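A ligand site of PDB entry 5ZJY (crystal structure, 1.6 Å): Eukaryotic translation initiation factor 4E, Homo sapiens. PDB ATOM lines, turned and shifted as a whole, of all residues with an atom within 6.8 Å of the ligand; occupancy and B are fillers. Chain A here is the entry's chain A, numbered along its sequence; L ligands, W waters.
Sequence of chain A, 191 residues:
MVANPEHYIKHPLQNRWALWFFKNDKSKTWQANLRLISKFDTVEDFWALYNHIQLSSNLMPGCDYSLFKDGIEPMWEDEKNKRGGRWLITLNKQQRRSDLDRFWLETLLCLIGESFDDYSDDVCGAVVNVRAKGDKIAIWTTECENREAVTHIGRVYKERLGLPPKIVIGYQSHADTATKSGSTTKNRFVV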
ATOM      1  N   PHE A  22       4.980 -17.797  13.341  1.00  0.00           N
ATOM      2  CA  PHE A  22       5.143 -18.544  14.579  1.00  0.00           C
ATOM      3  C   PHE A  22       4.479 -19.894  14.313  1.00  0.00           C
ATOM      4  O   PHE A  22       3.300 -19.940  13.984  1.00  0.00           O
ATOM      5  CB  PHE A  22       4.479 -17.812  15.726  1.00  0.00           C
ATOM      6  CG  PHE A  22       4.539 -18.575  17.031  1.00  0.00           C
ATOM      7  CD1 PHE A  22       3.613 -19.572  17.300  1.00  0.00           C
ATOM      8  CD2 PHE A  22       5.554 -18.307  17.948  1.00  0.00           C
ATOM      9  CE1 PHE A  22       3.686 -20.286  18.495  1.00  0.00           C
ATOM     10  CE2 PHE A  22       5.622 -19.009  19.135  1.00  0.00           C
ATOM     11  CZ  PHE A  22       4.700 -19.997  19.404  1.00  0.00           C
ATOM     12  N   TRP A  30       8.961 -20.708  23.304  1.00  0.00           N
ATOM     13  CA  TRP A  30       8.192 -19.754  22.480  1.00  0.00           C
ATOM     14  C   TRP A  30       9.096 -19.051  21.458  1.00  0.00           C
ATOM     15  O   TRP A  30       8.817 -19.093  20.250  1.00  0.00           O
ATOM     16  CB  TRP A  30       7.448 -18.725  23.350  1.00  0.00           C
ATOM     17  CG  TRP A  30       6.501 -17.851  22.555  1.00  0.00           C
ATOM     18  CD1 TRP A  30       5.196 -18.097  22.256  1.00  0.00           C
ATOM     19  CD2 TRP A  30       6.811 -16.589  21.950  1.00  0.00           C
ATOM     20  NE1 TRP A  30       4.663 -17.073  21.505  1.00  0.00           N
ATOM     21  CE2 TRP A  30       5.647 -16.141  21.290  1.00  0.00           C
ATOM     22  CE3 TRP A  30       7.970 -15.804  21.881  1.00  0.00           C
ATOM     23  CZ2 TRP A  30       5.600 -14.925  20.587  1.00  0.00           C
ATOM     24  CZ3 TRP A  30       7.928 -14.599  21.186  1.00  0.00           C
ATOM     25  CH2 TRP A  30       6.750 -14.177  20.550  1.00  0.00           C
ATOM     26  N   GLN A  31      10.194 -18.458  21.903  1.00  0.00           N
ATOM     27  CA  GLN A  31      11.111 -17.762  20.973  1.00  0.00           C
ATOM     28  C   GLN A  31      11.670 -18.619  19.835  1.00  0.00           C
ATOM     29  O   GLN A  31      11.849 -18.122  18.726  1.00  0.00           O
ATOM     30  CB  GLN A  31      12.254 -17.084  21.729  1.00  0.00           C
ATOM     31  CG  GLN A  31      11.828 -15.883  22.560  1.00  0.00           C
ATOM     32  CD  GLN A  31      13.003 -15.058  23.056  1.00  0.00           C
ATOM     33  OE1 GLN A  31      14.099 -15.109  22.508  1.00  0.00           O
ATOM     34  NE2 GLN A  31      12.763 -14.273  24.102  1.00  0.00           N
ATOM     35  N   GLY A  62      -2.930 -21.940  16.854  1.00  0.00           N
ATOM     36  CA  GLY A  62      -1.702 -21.700  17.580  1.00  0.00           C
ATOM     37  C   GLY A  62      -0.604 -21.006  16.782  1.00  0.00           C
ATOM     38  O   GLY A  62       0.408 -20.585  17.372  1.00  0.00           O
ATOM     39  N   ASP A  64       0.898 -17.947  14.191  1.00  0.00           N
ATOM     40  CA  ASP A  64       0.778 -16.498  14.039  1.00  0.00           C
ATOM     41  C   ASP A  64       1.521 -16.036  12.796  1.00  0.00           C
ATOM     42  O   ASP A  64       2.483 -16.668  12.340  1.00  0.00           O
ATOM     43  CB  ASP A  64       1.449 -15.699  15.185  1.00  0.00           C
ATOM     44  CG  ASP A  64       1.129 -16.203  16.579  1.00  0.00           C
ATOM     45  OD1 ASP A  64      -0.002 -16.653  16.892  1.00  0.00           O
ATOM     46  OD2 ASP A  64       2.021 -16.050  17.436  1.00  0.00           O
ATOM     47  N   PRO A  74       9.201  -9.501  17.009  1.00  0.00           N
ATOM     48  CA  PRO A  74       7.771  -9.460  17.334  1.00  0.00           C
ATOM     49  C   PRO A  74       7.480 -10.101  18.704  1.00  0.00           C
ATOM     50  O   PRO A  74       6.666 -11.008  18.823  1.00  0.00           O
ATOM     51  CB  PRO A  74       7.142 -10.240  16.190  1.00  0.00           C
ATOM     52  CG  PRO A  74       8.176 -11.212  15.822  1.00  0.00           C
ATOM     53  CD  PRO A  74       9.483 -10.516  15.991  1.00  0.00           C
ATOM     54  N   MET A  75       8.172  -9.581  19.719  1.00  0.00           N
ATOM     55  CA  MET A  75       8.086 -10.108  21.070  1.00  0.00           C
ATOM     56  C   MET A  75       8.135  -8.983  22.091  1.00  0.00           C
ATOM     57  O   MET A  75       8.739  -7.928  21.851  1.00  0.00           O
ATOM     58  CB  MET A  75       9.208 -11.109  21.320  1.00  0.00           C
ATOM     59  CG  MET A  75      10.621 -10.559  21.252  1.00  0.00           C
ATOM     60  SD  MET A  75      11.773 -11.891  21.672  1.00  0.00           S
ATOM     61  CE  MET A  75      11.644 -12.921  20.227  1.00  0.00           C
ATOM     62  N   TRP A  76       7.483  -9.219  23.228  1.00  0.00           N
ATOM     63  CA  TRP A  76       7.415  -8.251  24.326  1.00  0.00           C
ATOM     64  C   TRP A  76       8.779  -7.714  24.697  1.00  0.00           C
ATOM     65  O   TRP A  76       8.935  -6.523  24.978  1.00  0.00           O
ATOM     66  CB  TRP A  76       6.854  -8.923  25.596  1.00  0.00           C
ATOM     67  CG  TRP A  76       5.494  -9.515  25.483  1.00  0.00           C
ATOM     68  CD1 TRP A  76       4.431  -9.018  24.782  1.00  0.00           C
ATOM     69  CD2 TRP A  76       5.041 -10.699  26.134  1.00  0.00           C
ATOM     70  NE1 TRP A  76       3.336  -9.836  24.939  1.00  0.00           N
ATOM     71  CE2 TRP A  76       3.678 -10.879  25.781  1.00  0.00           C
ATOM     72  CE3 TRP A  76       5.638 -11.640  26.989  1.00  0.00           C
ATOM     73  CZ2 TRP A  76       2.916 -11.953  26.245  1.00  0.00           C
ATOM     74  CZ3 TRP A  76       4.866 -12.722  27.447  1.00  0.00           C
ATOM     75  CH2 TRP A  76       3.536 -12.862  27.067  1.00  0.00           C
ATOM     76  N   GLU A  77       9.767  -8.600  24.698  1.00  0.00           N
ATOM     77  CA  GLU A  77      11.110  -8.295  25.232  1.00  0.00           C
ATOM     78  C   GLU A  77      11.935  -7.331  24.419  1.00  0.00           C
ATOM     79  O   GLU A  77      12.930  -6.775  24.926  1.00  0.00           O
ATOM     80  CB  GLU A  77      11.924  -9.589  25.371  1.00  0.00           C
ATOM     81  CG  GLU A  77      11.340 -10.569  26.367  1.00  0.00           C
ATOM     82  CD  GLU A  77      10.552 -11.661  25.710  1.00  0.00           C
ATOM     83  OE1 GLU A  77       9.690 -11.354  24.834  1.00  0.00           O
ATOM     84  OE2 GLU A  77      10.767 -12.832  26.044  1.00  0.00           O
ATOM     85  N   ARG A  86      -0.661  -3.056  22.991  1.00  0.00           N
ATOM     86  CA  ARG A  86      -1.375  -3.398  21.770  1.00  0.00           C
ATOM     87  C   ARG A  86      -2.818  -2.987  21.823  1.00  0.00           C
ATOM     88  O   ARG A  86      -3.478  -3.058  22.889  1.00  0.00           O
ATOM     89  CB  ARG A  86      -1.237  -4.879  21.460  1.00  0.00           C
ATOM     90  CG  ARG A  86      -1.841  -5.775  22.517  1.00  0.00           C
ATOM     91  CD  ARG A  86      -1.758  -7.240  22.197  1.00  0.00           C
ATOM     92  NE  ARG A  86      -2.485  -7.975  23.238  1.00  0.00           N
ATOM     93  CZ  ARG A  86      -2.699  -9.284  23.224  1.00  0.00           C
ATOM     94  NH1 ARG A  86      -2.276 -10.016  22.214  1.00  0.00           N
ATOM     95  NH2 ARG A  86      -3.348  -9.856  24.234  1.00  0.00           N
ATOM     96  N   VAL A 127       0.177  -8.259  14.661  1.00  0.00           N
ATOM     97  CA  VAL A 127       0.206  -9.686  14.878  1.00  0.00           C
ATOM     98  C   VAL A 127      -1.210 -10.239  14.655  1.00  0.00           C
ATOM     99  O   VAL A 127      -2.177  -9.655  15.136  1.00  0.00           O
ATOM    100  CB  VAL A 127       0.606 -10.016  16.341  1.00  0.00           C
ATOM    101  CG1 VAL A 127       0.565 -11.513  16.604  1.00  0.00           C
ATOM    102  CG2 VAL A 127       1.979  -9.442  16.681  1.00  0.00           C
ATOM    103  N   ASN A 129      -3.163 -13.815  15.474  1.00  0.00           N
ATOM    104  CA  ASN A 129      -3.112 -15.106  16.166  1.00  0.00           C
ATOM    105  C   ASN A 129      -4.288 -15.941  15.684  1.00  0.00           C
ATOM    106  O   ASN A 129      -5.405 -15.516  15.846  1.00  0.00           O
ATOM    107  CB  ASN A 129      -3.231 -14.949  17.693  1.00  0.00           C
ATOM    108  CG  ASN A 129      -2.246 -13.952  18.300  1.00  0.00           C
ATOM    109  OD1 ASN A 129      -2.687 -12.983  18.929  1.00  0.00           O
ATOM    110  ND2 ASN A 129      -0.960 -14.213  18.219  1.00  0.00           N
ATOM    111  N   ARG A 131      -6.486 -18.913  16.576  1.00  0.00           N
ATOM    112  CA  ARG A 131      -6.731 -19.575  17.857  1.00  0.00           C
ATOM    113  C   ARG A 131      -8.118 -20.200  17.891  1.00  0.00           C
ATOM    114  O   ARG A 131      -9.107 -19.600  17.441  1.00  0.00           O
ATOM    115  CB  ARG A 131      -6.619 -18.603  19.043  1.00  0.00           C
ATOM    116  CG  ARG A 131      -5.234 -18.009  19.281  1.00  0.00           C
ATOM    117  CD  ARG A 131      -4.204 -19.021  19.712  1.00  0.00           C
ATOM    118  NE  ARG A 131      -2.887 -18.415  19.970  1.00  0.00           N
ATOM    119  CZ  ARG A 131      -1.974 -18.137  19.040  1.00  0.00           C
ATOM    120  NH1 ARG A 131      -2.189 -18.362  17.757  1.00  0.00           N
ATOM    121  NH2 ARG A 131      -0.835 -17.583  19.411  1.00  0.00           N
ATOM    122  N   LYS A 133     -10.053 -20.508  20.469  1.00  0.00           N
ATOM    123  CA  LYS A 133     -10.953 -19.686  21.308  1.00  0.00           C
ATOM    124  C   LYS A 133     -11.386 -18.369  20.660  1.00  0.00           C
ATOM    125  O   LYS A 133     -12.215 -17.675  21.228  1.00  0.00           O
ATOM    126  CB  LYS A 133     -10.285 -19.384  22.649  1.00  0.00           C
ATOM    127  N   GLY A 134     -10.808 -18.008  19.503  1.00  0.00           N
ATOM    128  CA  GLY A 134     -11.164 -16.791  18.818  1.00  0.00           C
ATOM    129  C   GLY A 134      -9.883 -16.197  18.262  1.00  0.00           C
ATOM    130  O   GLY A 134      -8.862 -16.137  18.961  1.00  0.00           O
ATOM    131  N   LYS A 136      -7.280 -13.352  16.916  1.00  0.00           N
ATOM    132  CA  LYS A 136      -6.968 -12.024  17.410  1.00  0.00           C
ATOM    133  C   LYS A 136      -6.093 -11.314  16.363  1.00  0.00           C
ATOM    134  O   LYS A 136      -5.209 -11.914  15.756  1.00  0.00           O
ATOM    135  CB  LYS A 136      -6.238 -12.119  18.743  1.00  0.00           C
ATOM    136  CG  LYS A 136      -7.119 -12.611  19.873  1.00  0.00           C
ATOM    137  CD  LYS A 136      -6.333 -12.799  21.163  1.00  0.00           C
ATOM    138  CE  LYS A 136      -5.516 -14.065  21.150  1.00  0.00           C
ATOM    139  NZ  LYS A 136      -4.871 -14.239  22.482  1.00  0.00           N
ATOM    140  N   TRP A 140       0.701  -3.301  17.595  1.00  0.00           N
ATOM    141  CA  TRP A 140       1.649  -3.052  18.677  1.00  0.00           C
ATOM    142  C   TRP A 140       2.332  -1.677  18.541  1.00  0.00           C
ATOM    143  O   TRP A 140       2.812  -1.343  17.459  1.00  0.00           O
ATOM    144  CB  TRP A 140       2.714  -4.120  18.666  1.00  0.00           C
ATOM    145  CG  TRP A 140       2.284  -5.505  19.111  1.00  0.00           C
ATOM    146  CD1 TRP A 140       1.062  -6.100  18.963  1.00  0.00           C
ATOM    147  CD2 TRP A 140       3.117  -6.450  19.771  1.00  0.00           C
ATOM    148  NE1 TRP A 140       1.107  -7.371  19.498  1.00  0.00           N
ATOM    149  CE2 TRP A 140       2.354  -7.605  19.997  1.00  0.00           C
ATOM    150  CE3 TRP A 140       4.444  -6.431  20.200  1.00  0.00           C
ATOM    151  CZ2 TRP A 140       2.867  -8.737  20.635  1.00  0.00           C
ATOM    152  CZ3 TRP A 140       4.963  -7.557  20.801  1.00  0.00           C
ATOM    153  CH2 TRP A 140       4.166  -8.702  21.022  1.00  0.00           C
ATOM    154  N   THR A 177      -0.160  -7.735  30.258  1.00  0.00           N
ATOM    155  CA  THR A 177      -0.474  -9.031  29.634  1.00  0.00           C
ATOM    156  C   THR A 177       0.456 -10.144  30.123  1.00  0.00           C
ATOM    157  O   THR A 177       0.010 -11.267  30.379  1.00  0.00           O
ATOM    158  CB  THR A 177      -0.361  -8.967  28.097  1.00  0.00           C
ATOM    159  OG1 THR A 177      -1.227  -7.936  27.607  1.00  0.00           O
ATOM    160  CG2 THR A 177      -0.722 -10.291  27.458  1.00  0.00           C
HETATM  161  P1  LIG L   1      -0.466 -15.844  22.925  1.00  0.00           P
HETATM  162  O1  LIG L   1      -0.127 -16.866  21.902  1.00  0.00           O
HETATM  163  O2  LIG L   1      -0.216 -14.390  22.657  1.00  0.00           O
HETATM  164  O3  LIG L   1      -1.984 -15.920  23.429  1.00  0.00           O
HETATM  165  O4  LIG L   1       0.315 -16.192  24.301  1.00  0.00           O
HETATM  166  P2  LIG L   1      -2.981 -17.190  23.413  1.00  0.00           P
HETATM  167  O5  LIG L   1      -2.265 -18.386  22.838  1.00  0.00           O
HETATM  168  O6  LIG L   1      -4.225 -16.765  22.698  1.00  0.00           O
HETATM  169  O7  LIG L   1      -3.194 -17.369  24.973  1.00  0.00           O
HETATM  170  P3  LIG L   1      -3.792 -16.238  25.966  1.00  0.00           P
HETATM  171  O8  LIG L   1      -4.210 -15.057  25.124  1.00  0.00           O
HETATM  172  O9  LIG L   1      -2.610 -15.958  26.880  1.00  0.00           O
HETATM  173  O10 LIG L   1      -4.967 -16.942  26.601  1.00  0.00           O
HETATM  174  C1  LIG L   1       0.461 -17.529  24.779  1.00  0.00           C
HETATM  175  C2  LIG L   1       1.807 -17.736  25.466  1.00  0.00           C
HETATM  176  O11 LIG L   1       2.872 -17.610  24.521  1.00  0.00           O
HETATM  177  C3  LIG L   1       2.117 -16.747  26.567  1.00  0.00           C
HETATM  178  O12 LIG L   1       1.542 -17.145  27.804  1.00  0.00           O
HETATM  179  C4  LIG L   1       3.633 -16.746  26.572  1.00  0.00           C
HETATM  180  O13 LIG L   1       4.185 -17.899  27.221  1.00  0.00           O
HETATM  181  C5  LIG L   1       3.974 -16.923  25.110  1.00  0.00           C
HETATM  182  N1  LIG L   1       4.216 -15.611  24.473  1.00  0.00           N
HETATM  183  C6  LIG L   1       3.386 -14.866  23.694  1.00  0.00           C
HETATM  184  N2  LIG L   1       3.987 -13.707  23.300  1.00  0.00           N
HETATM  185  C7  LIG L   1       3.380 -12.657  22.455  1.00  0.00           C
HETATM  186  C8  LIG L   1       5.211 -13.733  23.819  1.00  0.00           C
HETATM  187  C9  LIG L   1       6.360 -12.818  23.766  1.00  0.00           C
HETATM  188  O14 LIG L   1       6.323 -11.735  23.140  1.00  0.00           O
HETATM  189  N3  LIG L   1       7.457 -13.180  24.450  1.00  0.00           N
HETATM  190  C10 LIG L   1       7.540 -14.345  25.139  1.00  0.00           C
HETATM  191  N4  LIG L   1       8.675 -14.648  25.795  1.00  0.00           N
HETATM  192  N5  LIG L   1       6.531 -15.227  25.226  1.00  0.00           N
HETATM  193  C11 LIG L   1       5.363 -14.964  24.597  1.00  0.00           C
HETATM  194  O   HOH W   1      -1.998 -19.729  26.086  1.00  0.00           O
HETATM  195  O   HOH W   2       2.661 -20.600  23.152  1.00  0.00           O
HETATM  196  O   HOH W   3      -5.900 -14.195  28.324  1.00  0.00           O
HETATM  197  O   HOH W   4      -6.518 -18.007  22.711  1.00  0.00           O
HETATM  198  O   HOH W   5      -0.435 -12.708  24.788  1.00  0.00           O
HETATM  199  O   HOH W   6      -0.563 -14.189  27.029  1.00  0.00           O
HETATM  200  O   HOH W   7       4.554 -20.432  26.035  1.00  0.00           O
HETATM  201  O   HOH W   8      -2.260 -12.843  21.526  1.00  0.00           O
HETATM  202  O   HOH W   9       1.546 -18.954  21.674  1.00  0.00           O
HETATM  203  O   HOH W  10       2.232 -13.150  19.385  1.00  0.00           O
HETATM  204  O   HOH W  11       2.287 -16.652  19.972  1.00  0.00           O
HETATM  205  O   HOH W  12       0.599 -11.619  20.811  1.00  0.00           O
HETATM  206  O   HOH W  13      -3.127 -12.673  24.707  1.00  0.00           O
HETATM  207  O   HOH W  14       9.206 -17.604  26.755  1.00  0.00           O
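An oxygen (O6) of the ligand is in salt-bridge range of the side-chain amino group (NZ) of Lys 136, at 2.6 Å. The guanidinium group (NH2) of Arg 131 is in salt-bridge range of an oxygen (O1) of the ligand (2.7 Å). An oxygen (O14) of the ligand lies within hydrogen-bond range of the backbone NH (N) of Trp 76 (2.8 Å). The side-chain carboxylate (OE2) of Glu 77 is in hydrogen-bond range of a nitrogen (N4) of the ligand (2.8 Å).
The backbone carbonyl oxygen of Lys 136 is in hydrogen-bond range of the backbone NH of Asn 129. The side-chain carboxylate (OD1) of Asp 64 is in salt-bridge range of the guanidinium group (NH2) of Arg 131 (2.8 Å). NH1 of Arg 131 sits close to O of Gly 62 (3.4 Å). NE2 of Gln 31 sits at hydrogen-bond distance from OE2 of Glu 77, 3.1 Å away. The side-chain sulfur (SD) of Met 75 is in hydrogen-bond range of the side-chain amide nitrogen (NE2) of Gln 31 (3.5 Å).
NE1 of Trp 30 lies close to N1 of the ligand (3.3 Å). Met 75 touches the ligand (CA to O14, 3.2 Å). Hydrophobic or aromatic side chains within 4 Å of the ligand: Trp 30, Met 75 and Trp 76. Within 4 Å of the ligand: Trp 30, Met 75, Trp 76, Glu 77, Arg 131 and Lys 136. The nearest printed residue that does not touch the ligand is Trp 140 (4.3 Å).
Water W13 lies within hydrogen-bond range of an oxygen (O8) of the ligand (2.7 Å), the guanidinium group (NH2) of Arg 86 (2.9 Å) and the side-chain amino group (NZ) of Lys 136 (3.2 Å). Water W8 lies within hydrogen-bond range of OD1 of Asn 129 (2.6 Å), O2 of the ligand (2.8 Å), NH1 of Arg 86 (2.9 Å) and NZ of Lys 136 (3.1 Å). Water W11 lies within hydrogen-bond range of the side-chain carboxylate of Asp 64 (2.6 Å), the indole nitrogen of Trp 30 (2.9 Å), an oxygen (O1) of the ligand (3.1 Å) and the guanidinium group of Arg 131 (3.3 Å).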
